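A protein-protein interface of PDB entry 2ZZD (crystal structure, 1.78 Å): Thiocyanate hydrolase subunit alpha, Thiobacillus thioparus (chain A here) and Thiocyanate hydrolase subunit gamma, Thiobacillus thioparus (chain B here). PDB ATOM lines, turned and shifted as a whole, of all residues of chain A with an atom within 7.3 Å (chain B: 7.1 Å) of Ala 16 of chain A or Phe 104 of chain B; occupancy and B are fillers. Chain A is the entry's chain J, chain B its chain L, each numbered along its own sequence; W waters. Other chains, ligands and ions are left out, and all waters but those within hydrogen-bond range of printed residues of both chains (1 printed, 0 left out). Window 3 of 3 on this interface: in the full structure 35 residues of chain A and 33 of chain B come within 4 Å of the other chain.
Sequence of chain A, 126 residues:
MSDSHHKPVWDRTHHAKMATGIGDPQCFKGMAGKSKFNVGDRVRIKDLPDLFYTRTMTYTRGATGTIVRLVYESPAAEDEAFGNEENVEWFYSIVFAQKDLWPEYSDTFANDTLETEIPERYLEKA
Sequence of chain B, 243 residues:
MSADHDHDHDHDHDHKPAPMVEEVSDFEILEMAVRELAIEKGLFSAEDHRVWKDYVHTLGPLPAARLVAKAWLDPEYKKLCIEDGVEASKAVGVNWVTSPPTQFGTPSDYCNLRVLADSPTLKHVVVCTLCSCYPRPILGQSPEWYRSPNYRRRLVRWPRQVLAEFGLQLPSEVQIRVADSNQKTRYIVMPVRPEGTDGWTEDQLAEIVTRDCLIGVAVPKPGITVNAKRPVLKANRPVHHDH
Among the printed residues, merely in contact across the chains: Ala 19 of chain A with Phe 104 of chain B, Asp 24 of chain A with Tyr 110 of chain B, Ile 22 of chain A with Val 97 of chain B, Thr 20 of chain A with Phe 104 of chain B, Thr 20 of chain A with Gln 103 of chain B, His 15 of chain A with Phe 104 of chain B, Gly 23 of chain A with Cys 111 of chain B, Ala 16 of chain A with Phe 104 of chain B, Gly 23 of chain A with Phe 104 of chain B, Gly 23 of chain A with Val 97 of chain B, Asp 24 of chain A with Phe 104 of chain B and Gly 21 of chain A with Val 97 of chain B.
Ala 16 of chain A touches one residue of chain B.
Printed residues of chain B within 4 Å of Gln 26 of chain A: Cys 111 (3.0 Å).
Phe 104 of chain B touches six residues of chain A.
No residue of chain A comes within 4 Å of Gly 105 of chain B.
Printed residues of chain A within 4 Å of Cys 111 of chain B: Gly 23, Asp 24 and Gln 26.
The nearest residue of chain B that does not touch Ala 16 of chain A is Thr 102 of chain B (6.2 Å).
The nearest residue of chain A that does not touch Phe 104 of chain B is Gly 21 of chain A (4.7 Å).
The nearest printed residue of chain B that does not touch Gly 21 of chain A is Phe 104 of chain B (4.7 Å).
Hydrophobic or aromatic side chains of chain A within 4 Å of the printed part of chain B: His 15, Ala 16 and Ala 19.
Of the 14 printed residues of chain B, 5 touch a printed residue of chain A.
Among the printed residues, no Asp or Glu carboxylate lies within 4 Å of a Lys or Arg side-chain nitrogen of the other chain.
OG1 of Thr 102 of chain B lies within hydrogen-bond range of N of Phe 104 of chain B, at 3.0 Å.
OG1 of Thr 20 of chain A sits at hydrogen-bond distance from O of Ala 16 of chain A, 2.6 Å away.
The backbone NH of Asp 24 of chain A lies close to the side-chain amide oxygen of Gln 26 of chain A (3.5 Å).
The backbone carbonyl oxygen (O) of Trp 96 of chain B lies within hydrogen-bond range of the side-chain sulfur (SG) of Cys 111 of chain B, at 3.6 Å.
The side-chain sulfur of Cys 111 of chain B sits at hydrogen-bond distance from the backbone carbonyl oxygen of Phe 104 of chain B, 3.6 Å away.
The backbone NH of Phe 104 of chain B is in hydrogen-bond range of the backbone carbonyl oxygen of Val 97 of chain B (3.2 Å).
Water W1 lies within hydrogen-bond range of O of Cys 111 of chain B (3.1 Å) and NE2 of Gln 26 of chain A (3.3 Å).
O of Asp 24 of chain A is in hydrogen-bond range of N of Cys 111 of chain B (2.7 Å).
NE2 of Gln 26 of chain A lies within hydrogen-bond range of O of Cys 111 of chain B (3.0 Å).
N of Gly 21 of chain A sits at hydrogen-bond distance from O of Gln 103 of chain B (2.8 Å).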
ATOM      1  N   ARG A  12      18.684  27.126  27.923  1.00  0.00           N
ATOM      2  CA  ARG A  12      17.645  28.043  27.489  1.00  0.00           C
ATOM      3  C   ARG A  12      16.379  27.379  26.935  1.00  0.00           C
ATOM      4  O   ARG A  12      15.477  28.067  26.452  1.00  0.00           O
ATOM      5  CB  ARG A  12      18.237  29.036  26.481  1.00  0.00           C
ATOM      6  CG  ARG A  12      19.560  29.661  26.957  1.00  0.00           C
ATOM      7  CD  ARG A  12      19.811  31.030  26.340  1.00  0.00           C
ATOM      8  NE  ARG A  12      19.622  31.050  24.891  1.00  0.00           N
ATOM      9  CZ  ARG A  12      20.550  30.735  23.994  1.00  0.00           C
ATOM     10  NH1 ARG A  12      21.762  30.366  24.379  1.00  0.00           N
ATOM     11  NH2 ARG A  12      20.260  30.805  22.703  1.00  0.00           N
ATOM     12  N   THR A  13      16.295  26.053  27.030  1.00  0.00           N
ATOM     13  CA  THR A  13      15.113  25.345  26.534  1.00  0.00           C
ATOM     14  C   THR A  13      14.268  24.719  27.643  1.00  0.00           C
ATOM     15  O   THR A  13      13.116  24.358  27.411  1.00  0.00           O
ATOM     16  CB  THR A  13      15.492  24.213  25.554  1.00  0.00           C
ATOM     17  OG1 THR A  13      16.227  23.201  26.253  1.00  0.00           O
ATOM     18  CG2 THR A  13      16.328  24.754  24.417  1.00  0.00           C
ATOM     19  N   HIS A  14      14.830  24.599  28.844  1.00  0.00           N
ATOM     20  CA  HIS A  14      14.112  23.984  29.958  1.00  0.00           C
ATOM     21  C   HIS A  14      12.700  24.501  30.249  1.00  0.00           C
ATOM     22  O   HIS A  14      11.758  23.716  30.338  1.00  0.00           O
ATOM     23  CB  HIS A  14      14.924  24.085  31.253  1.00  0.00           C
ATOM     24  CG  HIS A  14      14.178  23.607  32.462  1.00  0.00           C
ATOM     25  ND1 HIS A  14      13.980  22.271  32.736  1.00  0.00           N
ATOM     26  CD2 HIS A  14      13.520  24.290  33.429  1.00  0.00           C
ATOM     27  CE1 HIS A  14      13.231  22.151  33.818  1.00  0.00           C
ATOM     28  NE2 HIS A  14      12.938  23.362  34.258  1.00  0.00           N
ATOM     29  N   HIS A  15      12.557  25.812  30.422  1.00  0.00           N
ATOM     30  CA  HIS A  15      11.254  26.387  30.740  1.00  0.00           C
ATOM     31  C   HIS A  15      10.206  26.138  29.655  1.00  0.00           C
ATOM     32  O   HIS A  15       9.080  25.741  29.955  1.00  0.00           O
ATOM     33  CB  HIS A  15      11.381  27.893  30.993  1.00  0.00           C
ATOM     34  CG  HIS A  15      10.124  28.526  31.506  1.00  0.00           C
ATOM     35  ND1 HIS A  15       9.615  28.263  32.760  1.00  0.00           N
ATOM     36  CD2 HIS A  15       9.265  29.399  30.927  1.00  0.00           C
ATOM     37  CE1 HIS A  15       8.496  28.943  32.931  1.00  0.00           C
ATOM     38  NE2 HIS A  15       8.260  29.640  31.832  1.00  0.00           N
ATOM     39  N   ALA A  16      10.569  26.373  28.399  1.00  0.00           N
ATOM     40  CA  ALA A  16       9.628  26.168  27.302  1.00  0.00           C
ATOM     41  C   ALA A  16       9.221  24.701  27.179  1.00  0.00           C
ATOM     42  O   ALA A  16       8.055  24.389  26.935  1.00  0.00           O
ATOM     43  CB  ALA A  16      10.235  26.654  25.991  1.00  0.00           C
ATOM     44  N   LYS A  17      10.181  23.798  27.339  1.00  0.00           N
ATOM     45  CA  LYS A  17       9.879  22.376  27.240  1.00  0.00           C
ATOM     46  C   LYS A  17       8.920  21.937  28.336  1.00  0.00           C
ATOM     47  O   LYS A  17       8.047  21.099  28.115  1.00  0.00           O
ATOM     48  CB  LYS A  17      11.166  21.555  27.314  1.00  0.00           C
ATOM     49  CG  LYS A  17      11.989  21.681  26.056  1.00  0.00           C
ATOM     50  CD  LYS A  17      13.226  20.809  26.063  1.00  0.00           C
ATOM     51  CE  LYS A  17      13.765  20.717  24.644  1.00  0.00           C
ATOM     52  NZ  LYS A  17      15.178  20.266  24.567  1.00  0.00           N
ATOM     53  N   MET A  18       9.083  22.520  29.515  1.00  0.00           N
ATOM     54  CA  MET A  18       8.248  22.188  30.653  1.00  0.00           C
ATOM     55  C   MET A  18       6.857  22.820  30.617  1.00  0.00           C
ATOM     56  O   MET A  18       5.872  22.181  30.989  1.00  0.00           O
ATOM     57  CB  MET A  18       8.961  22.609  31.942  1.00  0.00           C
ATOM     58  CG  MET A  18       8.115  22.520  33.194  1.00  0.00           C
ATOM     59  SD  MET A  18       9.015  23.094  34.642  1.00  0.00           S
ATOM     60  CE  MET A  18       9.021  24.860  34.335  1.00  0.00           C
ATOM     61  N   ALA A  19       6.771  24.060  30.148  1.00  0.00           N
ATOM     62  CA  ALA A  19       5.494  24.771  30.149  1.00  0.00           C
ATOM     63  C   ALA A  19       4.684  24.859  28.859  1.00  0.00           C
ATOM     64  O   ALA A  19       3.494  25.161  28.912  1.00  0.00           O
ATOM     65  CB  ALA A  19       5.705  26.184  30.703  1.00  0.00           C
ATOM     66  N   THR A  20       5.297  24.616  27.707  1.00  0.00           N
ATOM     67  CA  THR A  20       4.543  24.727  26.462  1.00  0.00           C
ATOM     68  C   THR A  20       3.279  23.867  26.455  1.00  0.00           C
ATOM     69  O   THR A  20       3.322  22.670  26.755  1.00  0.00           O
ATOM     70  CB  THR A  20       5.424  24.379  25.246  1.00  0.00           C
ATOM     71  OG1 THR A  20       6.485  25.338  25.144  1.00  0.00           O
ATOM     72  CG2 THR A  20       4.602  24.415  23.962  1.00  0.00           C
ATOM     73  N   GLY A  21       2.154  24.499  26.122  1.00  0.00           N
ATOM     74  CA  GLY A  21       0.883  23.800  26.062  1.00  0.00           C
ATOM     75  C   GLY A  21       0.236  23.546  27.410  1.00  0.00           C
ATOM     76  O   GLY A  21      -0.882  23.033  27.475  1.00  0.00           O
ATOM     77  N   ILE A  22       0.931  23.904  28.487  1.00  0.00           N
ATOM     78  CA  ILE A  22       0.420  23.685  29.837  1.00  0.00           C
ATOM     79  C   ILE A  22       0.240  24.999  30.586  1.00  0.00           C
ATOM     80  O   ILE A  22      -0.807  25.239  31.194  1.00  0.00           O
ATOM     81  CB  ILE A  22       1.377  22.770  30.627  1.00  0.00           C
ATOM     82  CG1 ILE A  22       1.501  21.430  29.900  1.00  0.00           C
ATOM     83  CG2 ILE A  22       0.861  22.568  32.054  1.00  0.00           C
ATOM     84  CD1 ILE A  22       2.724  20.625  30.282  1.00  0.00           C
ATOM     85  N   GLY A  23       1.265  25.843  30.541  1.00  0.00           N
ATOM     86  CA  GLY A  23       1.194  27.125  31.215  1.00  0.00           C
ATOM     87  C   GLY A  23       1.975  27.172  32.514  1.00  0.00           C
ATOM     88  O   GLY A  23       2.426  26.148  33.025  1.00  0.00           O
ATOM     89  N   ASP A  24       2.129  28.386  33.035  1.00  0.00           N
ATOM     90  CA  ASP A  24       2.827  28.652  34.287  1.00  0.00           C
ATOM     91  C   ASP A  24       1.798  29.461  35.081  1.00  0.00           C
ATOM     92  O   ASP A  24       1.303  30.478  34.596  1.00  0.00           O
ATOM     93  CB  ASP A  24       4.077  29.502  33.985  1.00  0.00           C
ATOM     94  CG  ASP A  24       4.900  29.830  35.220  1.00  0.00           C
ATOM     95  OD1 ASP A  24       4.464  29.516  36.349  1.00  0.00           O
ATOM     96  OD2 ASP A  24       5.994  30.421  35.044  1.00  0.00           O
ATOM     97  N   PRO A  25       1.501  29.053  36.331  1.00  0.00           N
ATOM     98  CA  PRO A  25       2.035  27.935  37.117  1.00  0.00           C
ATOM     99  C   PRO A  25       1.421  26.539  36.945  1.00  0.00           C
ATOM    100  O   PRO A  25       1.696  25.659  37.758  1.00  0.00           O
ATOM    101  CB  PRO A  25       1.868  28.435  38.542  1.00  0.00           C
ATOM    102  CG  PRO A  25       0.504  29.071  38.470  1.00  0.00           C
ATOM    103  CD  PRO A  25       0.527  29.820  37.129  1.00  0.00           C
ATOM    104  N   GLN A  26       0.601  26.324  35.917  1.00  0.00           N
ATOM    105  CA  GLN A  26      -0.001  25.001  35.728  1.00  0.00           C
ATOM    106  C   GLN A  26       1.047  23.890  35.648  1.00  0.00           C
ATOM    107  O   GLN A  26       0.803  22.766  36.096  1.00  0.00           O
ATOM    108  CB  GLN A  26      -0.872  24.960  34.463  1.00  0.00           C
ATOM    109  CG  GLN A  26      -2.199  25.702  34.590  1.00  0.00           C
ATOM    110  CD  GLN A  26      -2.095  27.173  34.236  1.00  0.00           C
ATOM    111  OE1 GLN A  26      -1.021  27.769  34.312  1.00  0.00           O
ATOM    112  NE2 GLN A  26      -3.221  27.770  33.853  1.00  0.00           N
ATOM    113  N   TRP B  96      -5.250  32.200  28.081  1.00  0.00           N
ATOM    114  CA  TRP B  96      -4.015  32.614  28.735  1.00  0.00           C
ATOM    115  C   TRP B  96      -2.788  31.762  28.451  1.00  0.00           C
ATOM    116  O   TRP B  96      -1.657  32.237  28.572  1.00  0.00           O
ATOM    117  CB  TRP B  96      -4.253  32.751  30.240  1.00  0.00           C
ATOM    118  CG  TRP B  96      -5.080  33.960  30.536  1.00  0.00           C
ATOM    119  CD1 TRP B  96      -6.356  34.210  30.102  1.00  0.00           C
ATOM    120  CD2 TRP B  96      -4.660  35.136  31.239  1.00  0.00           C
ATOM    121  NE1 TRP B  96      -6.749  35.474  30.485  1.00  0.00           N
ATOM    122  CE2 TRP B  96      -5.728  36.062  31.184  1.00  0.00           C
ATOM    123  CE3 TRP B  96      -3.483  35.497  31.908  1.00  0.00           C
ATOM    124  CZ2 TRP B  96      -5.652  37.331  31.773  1.00  0.00           C
ATOM    125  CZ3 TRP B  96      -3.407  36.762  32.497  1.00  0.00           C
ATOM    126  CH2 TRP B  96      -4.487  37.661  32.424  1.00  0.00           C
ATOM    127  N   VAL B  97      -3.001  30.516  28.054  1.00  0.00           N
ATOM    128  CA  VAL B  97      -1.884  29.639  27.751  1.00  0.00           C
ATOM    129  C   VAL B  97      -1.514  29.668  26.264  1.00  0.00           C
ATOM    130  O   VAL B  97      -0.353  29.876  25.909  1.00  0.00           O
ATOM    131  CB  VAL B  97      -2.203  28.174  28.144  1.00  0.00           C
ATOM    132  CG1 VAL B  97      -1.060  27.250  27.724  1.00  0.00           C
ATOM    133  CG2 VAL B  97      -2.432  28.083  29.645  1.00  0.00           C
ATOM    134  N   THR B  98      -2.510  29.491  25.401  1.00  0.00           N
ATOM    135  CA  THR B  98      -2.273  29.425  23.957  1.00  0.00           C
ATOM    136  C   THR B  98      -2.390  30.680  23.092  1.00  0.00           C
ATOM    137  O   THR B  98      -1.980  30.654  21.932  1.00  0.00           O
ATOM    138  CB  THR B  98      -3.169  28.344  23.327  1.00  0.00           C
ATOM    139  OG1 THR B  98      -4.543  28.664  23.574  1.00  0.00           O
ATOM    140  CG2 THR B  98      -2.856  26.988  23.931  1.00  0.00           C
ATOM    141  N   SER B  99      -2.950  31.768  23.611  1.00  0.00           N
ATOM    142  CA  SER B  99      -3.061  32.975  22.790  1.00  0.00           C
ATOM    143  C   SER B  99      -1.724  33.692  22.588  1.00  0.00           C
ATOM    144  O   SER B  99      -1.438  34.183  21.493  1.00  0.00           O
ATOM    145  CB  SER B  99      -4.096  33.942  23.380  1.00  0.00           C
ATOM    146  OG  SER B  99      -5.412  33.437  23.205  1.00  0.00           O
ATOM    147  N   PRO B 100      -0.887  33.771  23.637  1.00  0.00           N
ATOM    148  CA  PRO B 100       0.408  34.448  23.481  1.00  0.00           C
ATOM    149  C   PRO B 100       1.339  33.621  22.585  1.00  0.00           C
ATOM    150  O   PRO B 100       1.202  32.401  22.505  1.00  0.00           O
ATOM    151  CB  PRO B 100       0.928  34.541  24.915  1.00  0.00           C
ATOM    152  CG  PRO B 100      -0.334  34.494  25.761  1.00  0.00           C
ATOM    153  CD  PRO B 100      -1.133  33.430  25.049  1.00  0.00           C
ATOM    154  N   PRO B 101       2.314  34.270  21.923  1.00  0.00           N
ATOM    155  CA  PRO B 101       3.261  33.587  21.030  1.00  0.00           C
ATOM    156  C   PRO B 101       4.014  32.404  21.641  1.00  0.00           C
ATOM    157  O   PRO B 101       4.369  31.457  20.943  1.00  0.00           O
ATOM    158  CB  PRO B 101       4.210  34.711  20.611  1.00  0.00           C
ATOM    159  CG  PRO B 101       3.335  35.922  20.660  1.00  0.00           C
ATOM    160  CD  PRO B 101       2.595  35.715  21.960  1.00  0.00           C
ATOM    161  N   THR B 102       4.258  32.465  22.946  1.00  0.00           N
ATOM    162  CA  THR B 102       4.994  31.419  23.657  1.00  0.00           C
ATOM    163  C   THR B 102       4.279  30.076  23.726  1.00  0.00           C
ATOM    164  O   THR B 102       4.918  29.022  23.762  1.00  0.00           O
ATOM    165  CB  THR B 102       5.245  31.819  25.112  1.00  0.00           C
ATOM    166  OG1 THR B 102       3.982  31.981  25.773  1.00  0.00           O
ATOM    167  CG2 THR B 102       6.027  33.123  25.188  1.00  0.00           C
ATOM    168  N   GLN B 103       2.954  30.132  23.776  1.00  0.00           N
ATOM    169  CA  GLN B 103       2.106  28.957  23.920  1.00  0.00           C
ATOM    170  C   GLN B 103       2.248  28.410  25.343  1.00  0.00           C
ATOM    171  O   GLN B 103       1.949  27.245  25.610  1.00  0.00           O
ATOM    172  CB  GLN B 103       2.436  27.864  22.902  1.00  0.00           C
ATOM    173  CG  GLN B 103       1.270  26.881  22.721  1.00  0.00           C
ATOM    174  CD  GLN B 103       1.622  25.660  21.886  1.00  0.00           C
ATOM    175  OE1 GLN B 103       2.442  25.734  20.976  1.00  0.00           O
ATOM    176  NE2 GLN B 103       0.986  24.529  22.189  1.00  0.00           N
ATOM    177  N   PHE B 104       2.751  29.249  26.248  1.00  0.00           N
ATOM    178  CA  PHE B 104       2.845  28.871  27.654  1.00  0.00           C
ATOM    179  C   PHE B 104       2.530  30.091  28.508  1.00  0.00           C
ATOM    180  O   PHE B 104       2.952  30.198  29.660  1.00  0.00           O
ATOM    181  CB  PHE B 104       4.210  28.229  28.025  1.00  0.00           C
ATOM    182  CG  PHE B 104       5.436  29.069  27.730  1.00  0.00           C
ATOM    183  CD1 PHE B 104       5.763  30.179  28.510  1.00  0.00           C
ATOM    184  CD2 PHE B 104       6.326  28.671  26.731  1.00  0.00           C
ATOM    185  CE1 PHE B 104       6.967  30.873  28.303  1.00  0.00           C
ATOM    186  CE2 PHE B 104       7.527  29.355  26.515  1.00  0.00           C
ATOM    187  CZ  PHE B 104       7.848  30.458  27.306  1.00  0.00           C
ATOM    188  N   GLY B 105       1.730  30.982  27.925  1.00  0.00           N
ATOM    189  CA  GLY B 105       1.345  32.216  28.582  1.00  0.00           C
ATOM    190  C   GLY B 105       2.473  33.216  28.419  1.00  0.00           C
ATOM    191  O   GLY B 105       3.601  32.820  28.118  1.00  0.00           O
ATOM    192  N   THR B 106       2.201  34.505  28.588  1.00  0.00           N
ATOM    193  CA  THR B 106       3.285  35.469  28.461  1.00  0.00           C
ATOM    194  C   THR B 106       4.233  35.201  29.623  1.00  0.00           C
ATOM    195  O   THR B 106       3.810  34.775  30.699  1.00  0.00           O
ATOM    196  CB  THR B 106       2.796  36.934  28.541  1.00  0.00           C
ATOM    197  OG1 THR B 106       2.198  37.177  29.820  1.00  0.00           O
ATOM    198  CG2 THR B 106       1.785  37.221  27.437  1.00  0.00           C
ATOM    199  N   PRO B 107       5.536  35.425  29.419  1.00  0.00           N
ATOM    200  CA  PRO B 107       6.493  35.185  30.500  1.00  0.00           C
ATOM    201  C   PRO B 107       6.197  36.001  31.754  1.00  0.00           C
ATOM    202  O   PRO B 107       6.368  35.512  32.873  1.00  0.00           O
ATOM    203  CB  PRO B 107       7.824  35.591  29.877  1.00  0.00           C
ATOM    204  CG  PRO B 107       7.626  35.271  28.418  1.00  0.00           C
ATOM    205  CD  PRO B 107       6.226  35.782  28.169  1.00  0.00           C
ATOM    206  N   TYR B 110       1.862  35.436  33.210  1.00  0.00           N
ATOM    207  CA  TYR B 110       1.515  34.075  33.622  1.00  0.00           C
ATOM    208  C   TYR B 110       0.129  33.608  33.194  1.00  0.00           C
ATOM    209  O   TYR B 110      -0.501  34.228  32.338  1.00  0.00           O
ATOM    210  CB  TYR B 110       1.674  33.931  35.135  1.00  0.00           C
ATOM    211  CG  TYR B 110       3.051  34.333  35.613  1.00  0.00           C
ATOM    212  CD1 TYR B 110       3.256  35.552  36.261  1.00  0.00           C
ATOM    213  CD2 TYR B 110       4.161  33.522  35.362  1.00  0.00           C
ATOM    214  CE1 TYR B 110       4.533  35.957  36.645  1.00  0.00           C
ATOM    215  CE2 TYR B 110       5.444  33.919  35.743  1.00  0.00           C
ATOM    216  CZ  TYR B 110       5.622  35.140  36.385  1.00  0.00           C
ATOM    217  OH  TYR B 110       6.883  35.543  36.769  1.00  0.00           O
ATOM    218  N   CYS B 111      -0.344  32.514  33.791  1.00  0.00           N
ATOM    219  CA  CYS B 111      -1.637  31.945  33.414  1.00  0.00           C
ATOM    220  C   CYS B 111      -2.613  31.719  34.565  1.00  0.00           C
ATOM    221  O   CYS B 111      -3.191  30.638  34.693  1.00  0.00           O
ATOM    222  CB  CYS B 111      -1.410  30.614  32.687  1.00  0.00           C
ATOM    223  SG  CYS B 111      -0.138  30.701  31.396  1.00  0.00           S
HETATM  224  O   HOH W   1      -3.051  28.572  37.029  1.00  0.00           O
